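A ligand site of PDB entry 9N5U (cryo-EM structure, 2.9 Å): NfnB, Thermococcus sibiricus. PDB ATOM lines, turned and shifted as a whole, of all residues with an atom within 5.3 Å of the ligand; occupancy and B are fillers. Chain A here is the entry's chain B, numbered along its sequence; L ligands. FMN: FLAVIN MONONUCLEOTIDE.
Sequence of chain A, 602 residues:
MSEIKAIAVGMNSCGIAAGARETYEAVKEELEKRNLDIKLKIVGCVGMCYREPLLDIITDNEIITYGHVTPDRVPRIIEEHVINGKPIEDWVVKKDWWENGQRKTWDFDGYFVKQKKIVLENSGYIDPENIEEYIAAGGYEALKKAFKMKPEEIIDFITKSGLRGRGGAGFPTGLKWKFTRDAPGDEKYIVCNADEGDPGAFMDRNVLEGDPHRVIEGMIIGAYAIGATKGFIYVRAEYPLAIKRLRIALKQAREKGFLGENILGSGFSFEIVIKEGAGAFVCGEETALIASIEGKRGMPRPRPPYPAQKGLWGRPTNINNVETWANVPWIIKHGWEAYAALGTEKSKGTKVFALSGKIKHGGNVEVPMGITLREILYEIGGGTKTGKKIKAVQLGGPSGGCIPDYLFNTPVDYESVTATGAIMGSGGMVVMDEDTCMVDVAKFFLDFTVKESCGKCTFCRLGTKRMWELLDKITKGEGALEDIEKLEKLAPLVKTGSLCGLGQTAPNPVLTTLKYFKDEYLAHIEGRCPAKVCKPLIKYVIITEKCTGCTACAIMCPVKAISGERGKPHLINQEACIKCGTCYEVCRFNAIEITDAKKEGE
ND2 of Asn 193 is in hydrogen-bond range of O4' of the ligand (3.1 Å).
The side-chain amide oxygen (OD1) of Asn 321 sits close to an oxygen (O2) of the ligand.
An oxygen (O2') of the ligand sits close to the backbone carbonyl oxygen (O) of Gly 284.
The side-chain hydroxyl (OG1) of Thr 324 lies within hydrogen-bond range of an oxygen (O3P) of the ligand, at 3.1 Å.
O of Asp 195 sits close to O4 of the ligand (2.6 Å).
The backbone NH (N) of Glu 196 lies close to an oxygen (O4) of the ligand.
The backbone NH (N) of Glu 286 is in hydrogen-bond range of an oxygen (O2') of the ligand (3.2 Å).
The backbone NH (N) of Asn 321 lies within hydrogen-bond range of an oxygen (O3P) of the ligand (3.3 Å).
The side-chain amino group (NZ) of Lys 176 is in salt-bridge range of an oxygen (O1P) of the ligand (2.7 Å).
O of Ile 319 lies close to O1P of the ligand, at 3.0 Å.
The side-chain amide oxygen (OD1) of Asn 320 lies close to an oxygen (O1P) of the ligand (2.9 Å).
The side-chain amino group (NZ) of Lys 176 lies within salt-bridge range of the side-chain carboxylate (OE2) of Glu 286.
NZ of Lys 176 lies within hydrogen-bond range of O of Ile 319, 2.5 Å away.
The side-chain amide nitrogen of Asn 193 lies within hydrogen-bond range of the backbone carbonyl oxygen of Gly 284, at 2.9 Å.
The side-chain amide nitrogen (ND2) of Asn 321 lies close to the backbone NH (N) of Gly 167 (3.3 Å).
The backbone NH (N) of Gly 165 is in hydrogen-bond range of the backbone carbonyl oxygen (O) of Phe 171.
O of Asn 320 lies within hydrogen-bond range of N of Asn 193 (2.8 Å).
The backbone carbonyl oxygen of Asn 193 lies close to the side-chain amide oxygen of Asn 321, at 3.2 Å.
The side-chain carboxylate (OD2) of Asp 195 lies within hydrogen-bond range of the backbone NH (N) of Gly 284, 3.1 Å away.
The backbone carbonyl oxygen (O) of Gly 167 sits close to a nitrogen (N1) of the ligand, 3.2 Å away.
Gly 165 touches the ligand (CA to O2P, 3.2 Å).
Arg 166 touches the ligand.
Gly 197 touches the ligand.
O of Phe 281 touches C6 of the ligand, 3.4 Å away.
OE1 of Glu 285 touches C8M of the ligand, 3.3 Å away.
Gly 501 touches the ligand (CA to C8M, 3.6 Å).
CB of Leu 502 touches C7M of the ligand (3.6 Å).
Within 4 Å of the ligand: Gly 165, Arg 166, Gly 167, Lys 176, Asn 193, Asp 195, Glu 196, Gly 197, Phe 281, Gly 284, Glu 285, Glu 286, Ile 319, Asn 320, Asn 321, Thr 324, Gly 501 and Leu 502.
Along chain A the residues within 4 Å of the ligand span positions 165 to 502.
The nearest printed residue that does not touch the ligand is Phe 171 (4.4 Å).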
ATOM      1  N   GLY A 165      37.724 -19.766  27.762  1.00  0.00           N
ATOM      2  CA  GLY A 165      36.554 -18.904  27.727  1.00  0.00           C
ATOM      3  C   GLY A 165      36.717 -17.637  28.541  1.00  0.00           C
ATOM      4  O   GLY A 165      37.070 -17.682  29.723  1.00  0.00           O
ATOM      5  N   ARG A 166      36.447 -16.503  27.916  1.00  0.00           N
ATOM      6  CA  ARG A 166      36.617 -15.209  28.553  1.00  0.00           C
ATOM      7  C   ARG A 166      35.354 -14.686  29.212  1.00  0.00           C
ATOM      8  O   ARG A 166      35.379 -13.590  29.777  1.00  0.00           O
ATOM      9  CB  ARG A 166      37.113 -14.184  27.530  1.00  0.00           C
ATOM     10  CG  ARG A 166      38.435 -14.552  26.892  1.00  0.00           C
ATOM     11  CD  ARG A 166      39.590 -14.303  27.824  1.00  0.00           C
ATOM     12  NE  ARG A 166      40.870 -14.502  27.166  1.00  0.00           N
ATOM     13  CZ  ARG A 166      41.634 -15.571  27.329  1.00  0.00           C
ATOM     14  NH1 ARG A 166      41.288 -16.559  28.136  1.00  0.00           N
ATOM     15  NH2 ARG A 166      42.781 -15.657  26.660  1.00  0.00           N
ATOM     16  N   GLY A 167      34.262 -15.429  29.154  1.00  0.00           N
ATOM     17  CA  GLY A 167      33.010 -15.004  29.752  1.00  0.00           C
ATOM     18  C   GLY A 167      32.677 -15.645  31.068  1.00  0.00           C
ATOM     19  O   GLY A 167      31.660 -15.292  31.673  1.00  0.00           O
ATOM     20  N   GLY A 168      33.509 -16.554  31.555  1.00  0.00           N
ATOM     21  CA  GLY A 168      33.154 -17.313  32.731  1.00  0.00           C
ATOM     22  C   GLY A 168      34.295 -18.143  33.284  1.00  0.00           C
ATOM     23  O   GLY A 168      35.417 -17.643  33.418  1.00  0.00           O
ATOM     24  N   ALA A 169      34.011 -19.399  33.611  1.00  0.00           N
ATOM     25  CA  ALA A 169      34.944 -20.263  34.316  1.00  0.00           C
ATOM     26  C   ALA A 169      36.197 -20.585  33.512  1.00  0.00           C
ATOM     27  O   ALA A 169      37.157 -21.099  34.085  1.00  0.00           O
ATOM     28  CB  ALA A 169      34.244 -21.567  34.720  1.00  0.00           C
ATOM     29  N   GLY A 170      36.206 -20.310  32.215  1.00  0.00           N
ATOM     30  CA  GLY A 170      37.400 -20.520  31.422  1.00  0.00           C
ATOM     31  C   GLY A 170      37.553 -21.914  30.870  1.00  0.00           C
ATOM     32  O   GLY A 170      38.645 -22.480  30.880  1.00  0.00           O
ATOM     33  N   PHE A 171      36.453 -22.485  30.390  1.00  0.00           N
ATOM     34  CA  PHE A 171      36.516 -23.792  29.742  1.00  0.00           C
ATOM     35  C   PHE A 171      37.294 -23.667  28.438  1.00  0.00           C
ATOM     36  O   PHE A 171      37.139 -22.675  27.712  1.00  0.00           O
ATOM     37  CB  PHE A 171      35.098 -24.310  29.483  1.00  0.00           C
ATOM     38  CG  PHE A 171      35.052 -25.760  29.124  1.00  0.00           C
ATOM     39  CD1 PHE A 171      35.255 -26.732  30.081  1.00  0.00           C
ATOM     40  CD2 PHE A 171      34.772 -26.152  27.832  1.00  0.00           C
ATOM     41  CE1 PHE A 171      35.194 -28.068  29.758  1.00  0.00           C
ATOM     42  CE2 PHE A 171      34.712 -27.490  27.495  1.00  0.00           C
ATOM     43  CZ  PHE A 171      34.931 -28.448  28.459  1.00  0.00           C
ATOM     44  N   THR A 173      38.302 -23.517  24.778  1.00  0.00           N
ATOM     45  CA  THR A 173      37.406 -23.243  23.669  1.00  0.00           C
ATOM     46  C   THR A 173      37.458 -24.339  22.614  1.00  0.00           C
ATOM     47  O   THR A 173      36.426 -24.690  22.023  1.00  0.00           O
ATOM     48  CB  THR A 173      37.749 -21.883  23.063  1.00  0.00           C
ATOM     49  OG1 THR A 173      37.649 -20.878  24.064  1.00  0.00           O
ATOM     50  CG2 THR A 173      36.787 -21.535  21.942  1.00  0.00           C
ATOM     51  N   LYS A 176      35.230 -27.117  23.575  1.00  0.00           N
ATOM     52  CA  LYS A 176      33.841 -26.756  23.371  1.00  0.00           C
ATOM     53  C   LYS A 176      33.446 -26.892  21.908  1.00  0.00           C
ATOM     54  O   LYS A 176      32.385 -27.449  21.567  1.00  0.00           O
ATOM     55  CB  LYS A 176      33.610 -25.333  23.867  1.00  0.00           C
ATOM     56  CG  LYS A 176      32.222 -25.038  24.375  1.00  0.00           C
ATOM     57  CD  LYS A 176      32.183 -23.692  25.047  1.00  0.00           C
ATOM     58  CE  LYS A 176      30.843 -23.440  25.690  1.00  0.00           C
ATOM     59  NZ  LYS A 176      30.781 -22.090  26.301  1.00  0.00           N
ATOM     60  N   ASN A 193      27.662 -14.632  22.978  1.00  0.00           N
ATOM     61  CA  ASN A 193      27.048 -14.164  24.222  1.00  0.00           C
ATOM     62  C   ASN A 193      27.494 -12.728  24.463  1.00  0.00           C
ATOM     63  O   ASN A 193      28.623 -12.477  24.872  1.00  0.00           O
ATOM     64  CB  ASN A 193      27.427 -15.075  25.387  1.00  0.00           C
ATOM     65  CG  ASN A 193      26.463 -14.968  26.546  1.00  0.00           C
ATOM     66  OD1 ASN A 193      25.654 -14.058  26.609  1.00  0.00           O
ATOM     67  ND2 ASN A 193      26.563 -15.911  27.481  1.00  0.00           N
ATOM     68  N   ASP A 195      25.440 -10.720  26.426  1.00  0.00           N
ATOM     69  CA  ASP A 195      24.505 -10.367  27.493  1.00  0.00           C
ATOM     70  C   ASP A 195      25.265 -10.064  28.789  1.00  0.00           C
ATOM     71  O   ASP A 195      25.030 -10.673  29.827  1.00  0.00           O
ATOM     72  CB  ASP A 195      23.481 -11.483  27.696  1.00  0.00           C
ATOM     73  CG  ASP A 195      22.395 -11.125  28.690  1.00  0.00           C
ATOM     74  OD1 ASP A 195      22.313  -9.945  29.099  1.00  0.00           O
ATOM     75  OD2 ASP A 195      21.622 -12.023  29.079  1.00  0.00           O
ATOM     76  N   GLU A 196      26.182  -9.102  28.719  1.00  0.00           N
ATOM     77  CA  GLU A 196      26.992  -8.790  29.895  1.00  0.00           C
ATOM     78  C   GLU A 196      26.107  -8.166  30.955  1.00  0.00           C
ATOM     79  O   GLU A 196      25.812  -6.967  30.922  1.00  0.00           O
ATOM     80  CB  GLU A 196      28.170  -7.880  29.528  1.00  0.00           C
ATOM     81  CG  GLU A 196      27.837  -6.739  28.614  1.00  0.00           C
ATOM     82  CD  GLU A 196      28.942  -5.706  28.600  1.00  0.00           C
ATOM     83  OE1 GLU A 196      29.952  -5.932  29.285  1.00  0.00           O
ATOM     84  OE2 GLU A 196      28.782  -4.683  27.912  1.00  0.00           O
ATOM     85  N   GLY A 197      25.665  -8.987  31.903  1.00  0.00           N
ATOM     86  CA  GLY A 197      24.827  -8.516  32.980  1.00  0.00           C
ATOM     87  C   GLY A 197      25.565  -7.949  34.161  1.00  0.00           C
ATOM     88  O   GLY A 197      24.925  -7.463  35.095  1.00  0.00           O
ATOM     89  N   ASP A 204      32.477  -5.925  26.704  1.00  0.00           N
ATOM     90  CA  ASP A 204      31.833  -6.622  25.591  1.00  0.00           C
ATOM     91  C   ASP A 204      31.153  -5.647  24.638  1.00  0.00           C
ATOM     92  O   ASP A 204      31.282  -5.778  23.411  1.00  0.00           O
ATOM     93  CB  ASP A 204      30.828  -7.641  26.117  1.00  0.00           C
ATOM     94  CG  ASP A 204      31.461  -8.661  27.037  1.00  0.00           C
ATOM     95  OD1 ASP A 204      32.684  -8.884  26.920  1.00  0.00           O
ATOM     96  OD2 ASP A 204      30.744  -9.250  27.860  1.00  0.00           O
ATOM     97  N   PHE A 281      20.237 -10.564  34.220  1.00  0.00           N
ATOM     98  CA  PHE A 281      21.579 -11.065  34.531  1.00  0.00           C
ATOM     99  C   PHE A 281      21.645 -12.576  34.453  1.00  0.00           C
ATOM    100  O   PHE A 281      22.715 -13.140  34.180  1.00  0.00           O
ATOM    101  CB  PHE A 281      22.002 -10.565  35.911  1.00  0.00           C
ATOM    102  CG  PHE A 281      23.354 -11.050  36.350  1.00  0.00           C
ATOM    103  CD1 PHE A 281      24.498 -10.513  35.793  1.00  0.00           C
ATOM    104  CD2 PHE A 281      23.485 -12.008  37.334  1.00  0.00           C
ATOM    105  CE1 PHE A 281      25.741 -10.940  36.190  1.00  0.00           C
ATOM    106  CE2 PHE A 281      24.733 -12.429  37.737  1.00  0.00           C
ATOM    107  CZ  PHE A 281      25.861 -11.895  37.166  1.00  0.00           C
ATOM    108  N   VAL A 282      20.525 -13.267  34.686  1.00  0.00           N
ATOM    109  CA  VAL A 282      20.511 -14.718  34.633  1.00  0.00           C
ATOM    110  C   VAL A 282      20.488 -15.230  33.193  1.00  0.00           C
ATOM    111  O   VAL A 282      20.891 -16.364  32.943  1.00  0.00           O
ATOM    112  CB  VAL A 282      19.328 -15.260  35.447  1.00  0.00           C
ATOM    113  CG1 VAL A 282      18.011 -14.938  34.759  1.00  0.00           C
ATOM    114  CG2 VAL A 282      19.463 -16.748  35.703  1.00  0.00           C
ATOM    115  N   GLY A 284      22.415 -14.461  30.866  1.00  0.00           N
ATOM    116  CA  GLY A 284      23.769 -14.721  30.400  1.00  0.00           C
ATOM    117  C   GLY A 284      24.228 -16.143  30.632  1.00  0.00           C
ATOM    118  O   GLY A 284      25.199 -16.576  30.009  1.00  0.00           O
ATOM    119  N   GLU A 285      23.559 -16.872  31.521  1.00  0.00           N
ATOM    120  CA  GLU A 285      23.797 -18.300  31.697  1.00  0.00           C
ATOM    121  C   GLU A 285      23.437 -19.039  30.410  1.00  0.00           C
ATOM    122  O   GLU A 285      22.532 -18.651  29.677  1.00  0.00           O
ATOM    123  CB  GLU A 285      22.985 -18.804  32.893  1.00  0.00           C
ATOM    124  CG  GLU A 285      22.608 -20.281  32.889  1.00  0.00           C
ATOM    125  CD  GLU A 285      23.665 -21.149  33.506  1.00  0.00           C
ATOM    126  OE1 GLU A 285      24.603 -20.604  34.126  1.00  0.00           O
ATOM    127  OE2 GLU A 285      23.569 -22.384  33.378  1.00  0.00           O
ATOM    128  N   GLU A 286      24.181 -20.119  30.132  1.00  0.00           N
ATOM    129  CA  GLU A 286      24.010 -20.845  28.875  1.00  0.00           C
ATOM    130  C   GLU A 286      22.578 -21.362  28.715  1.00  0.00           C
ATOM    131  O   GLU A 286      21.917 -21.073  27.706  1.00  0.00           O
ATOM    132  CB  GLU A 286      24.990 -22.010  28.808  1.00  0.00           C
ATOM    133  CG  GLU A 286      26.415 -21.634  28.538  1.00  0.00           C
ATOM    134  CD  GLU A 286      27.342 -22.832  28.508  1.00  0.00           C
ATOM    135  OE1 GLU A 286      26.929 -23.901  28.998  1.00  0.00           O
ATOM    136  OE2 GLU A 286      28.474 -22.703  28.016  1.00  0.00           O
ATOM    137  N   ILE A 319      28.049 -21.786  22.560  1.00  0.00           N
ATOM    138  CA  ILE A 319      27.875 -20.455  23.135  1.00  0.00           C
ATOM    139  C   ILE A 319      29.234 -19.999  23.638  1.00  0.00           C
ATOM    140  O   ILE A 319      29.798 -20.594  24.556  1.00  0.00           O
ATOM    141  CB  ILE A 319      26.827 -20.462  24.256  1.00  0.00           C
ATOM    142  CG1 ILE A 319      25.584 -21.226  23.819  1.00  0.00           C
ATOM    143  CG2 ILE A 319      26.466 -19.038  24.653  1.00  0.00           C
ATOM    144  CD1 ILE A 319      24.585 -21.447  24.917  1.00  0.00           C
ATOM    145  N   ASN A 320      29.751 -18.944  23.023  1.00  0.00           N
ATOM    146  CA  ASN A 320      31.026 -18.349  23.414  1.00  0.00           C
ATOM    147  C   ASN A 320      30.839 -16.860  23.628  1.00  0.00           C
ATOM    148  O   ASN A 320      29.895 -16.236  23.131  1.00  0.00           O
ATOM    149  CB  ASN A 320      32.115 -18.589  22.363  1.00  0.00           C
ATOM    150  CG  ASN A 320      32.870 -19.885  22.587  1.00  0.00           C
ATOM    151  OD1 ASN A 320      33.925 -19.897  23.209  1.00  0.00           O
ATOM    152  ND2 ASN A 320      32.328 -20.981  22.089  1.00  0.00           N
ATOM    153  N   ASN A 321      31.763 -16.278  24.392  1.00  0.00           N
ATOM    154  CA  ASN A 321      31.750 -14.868  24.724  1.00  0.00           C
ATOM    155  C   ASN A 321      32.240 -14.030  23.546  1.00  0.00           C
ATOM    156  O   ASN A 321      32.869 -14.524  22.612  1.00  0.00           O
ATOM    157  CB  ASN A 321      32.623 -14.633  25.963  1.00  0.00           C
ATOM    158  CG  ASN A 321      32.444 -13.260  26.566  1.00  0.00           C
ATOM    159  OD1 ASN A 321      31.416 -12.614  26.367  1.00  0.00           O
ATOM    160  ND2 ASN A 321      33.447 -12.804  27.302  1.00  0.00           N
ATOM    161  N   VAL A 322      31.938 -12.735  23.604  1.00  0.00           N
ATOM    162  CA  VAL A 322      32.387 -11.801  22.571  1.00  0.00           C
ATOM    163  C   VAL A 322      33.903 -11.751  22.519  1.00  0.00           C
ATOM    164  O   VAL A 322      34.502 -11.670  21.444  1.00  0.00           O
ATOM    165  CB  VAL A 322      31.793 -10.396  22.841  1.00  0.00           C
ATOM    166  CG1 VAL A 322      32.247  -9.411  21.792  1.00  0.00           C
ATOM    167  CG2 VAL A 322      30.286 -10.470  22.876  1.00  0.00           C
ATOM    168  N   THR A 324      36.100 -14.158  23.353  1.00  0.00           N
ATOM    169  CA  THR A 324      36.646 -15.370  22.763  1.00  0.00           C
ATOM    170  C   THR A 324      36.537 -15.348  21.240  1.00  0.00           C
ATOM    171  O   THR A 324      37.499 -15.670  20.517  1.00  0.00           O
ATOM    172  CB  THR A 324      35.927 -16.593  23.338  1.00  0.00           C
ATOM    173  OG1 THR A 324      35.909 -16.503  24.770  1.00  0.00           O
ATOM    174  CG2 THR A 324      36.613 -17.871  22.924  1.00  0.00           C
ATOM    175  N   CYS A 500      22.367 -22.941  39.567  1.00  0.00           N
ATOM    176  CA  CYS A 500      23.111 -22.260  38.514  1.00  0.00           C
ATOM    177  C   CYS A 500      24.226 -21.425  39.120  1.00  0.00           C
ATOM    178  O   CYS A 500      24.366 -21.319  40.334  1.00  0.00           O
ATOM    179  CB  CYS A 500      22.180 -21.407  37.652  1.00  0.00           C
ATOM    180  SG  CYS A 500      22.192 -19.646  38.017  1.00  0.00           S
ATOM    181  N   GLY A 501      25.036 -20.844  38.235  1.00  0.00           N
ATOM    182  CA  GLY A 501      26.224 -20.124  38.675  1.00  0.00           C
ATOM    183  C   GLY A 501      25.935 -18.811  39.380  1.00  0.00           C
ATOM    184  O   GLY A 501      26.803 -18.330  40.120  1.00  0.00           O
ATOM    185  N   LEU A 502      24.761 -18.221  39.155  1.00  0.00           N
ATOM    186  CA  LEU A 502      24.424 -16.985  39.855  1.00  0.00           C
ATOM    187  C   LEU A 502      24.354 -17.204  41.359  1.00  0.00           C
ATOM    188  O   LEU A 502      24.900 -16.410  42.135  1.00  0.00           O
ATOM    189  CB  LEU A 502      23.114 -16.408  39.339  1.00  0.00           C
ATOM    190  CG  LEU A 502      22.429 -15.251  40.091  1.00  0.00           C
ATOM    191  CD1 LEU A 502      23.383 -14.131  40.430  1.00  0.00           C
ATOM    192  CD2 LEU A 502      21.278 -14.700  39.284  1.00  0.00           C
HETATM  193  N1  FMN L   1      29.076 -15.363  29.838  1.00  0.00           N
HETATM  194  C2  FMN L   1      29.278 -14.321  28.971  1.00  0.00           C
HETATM  195  O2  FMN L   1      30.020 -14.476  28.002  1.00  0.00           O
HETATM  196  N3  FMN L   1      28.666 -13.104  29.172  1.00  0.00           N
HETATM  197  C4  FMN L   1      27.839 -12.946  30.262  1.00  0.00           C
HETATM  198  O4  FMN L   1      27.293 -11.884  30.468  1.00  0.00           O
HETATM  199  C4A FMN L   1      27.618 -13.987  31.141  1.00  0.00           C
HETATM  200  N5  FMN L   1      26.790 -13.818  32.222  1.00  0.00           N
HETATM  201  C5A FMN L   1      26.575 -14.855  33.094  1.00  0.00           C
HETATM  202  C6  FMN L   1      25.736 -14.682  34.181  1.00  0.00           C
HETATM  203  C7  FMN L   1      25.522 -15.733  35.047  1.00  0.00           C
HETATM  204  C7M FMN L   1      24.616 -15.551  36.220  1.00  0.00           C
HETATM  205  C8  FMN L   1      26.146 -16.954  34.841  1.00  0.00           C
HETATM  206  C8M FMN L   1      25.914 -18.092  35.780  1.00  0.00           C
HETATM  207  C9  FMN L   1      26.986 -17.128  33.755  1.00  0.00           C
HETATM  208  C9A FMN L   1      27.195 -16.072  32.872  1.00  0.00           C
HETATM  209  N10 FMN L   1      28.028 -16.248  31.793  1.00  0.00           N
HETATM  210  C10 FMN L   1      28.243 -15.211  30.921  1.00  0.00           C
HETATM  211  C1' FMN L   1      28.700 -17.555  31.563  1.00  0.00           C
HETATM  212  C2' FMN L   1      27.896 -18.396  30.583  1.00  0.00           C
HETATM  213  O2' FMN L   1      26.978 -19.193  31.309  1.00  0.00           O
HETATM  214  C3' FMN L   1      28.836 -19.295  29.802  1.00  0.00           C
HETATM  215  O3' FMN L   1      29.711 -19.924  30.697  1.00  0.00           O
HETATM  216  C4' FMN L   1      29.622 -18.494  28.782  1.00  0.00           C
HETATM  217  O4' FMN L   1      28.784 -18.082  27.741  1.00  0.00           O
HETATM  218  C5' FMN L   1      30.738 -19.353  28.226  1.00  0.00           C
HETATM  219  O5' FMN L   1      31.578 -18.576  27.410  1.00  0.00           O
HETATM  220  P   FMN L   1      32.913 -19.235  26.811  1.00  0.00           P
HETATM  221  O1P FMN L   1      32.526 -20.183  25.702  1.00  0.00           O
HETATM  222  O2P FMN L   1      33.606 -20.012  27.889  1.00  0.00           O
HETATM  223  O3P FMN L   1      33.799 -18.144  26.268  1.00  0.00           O
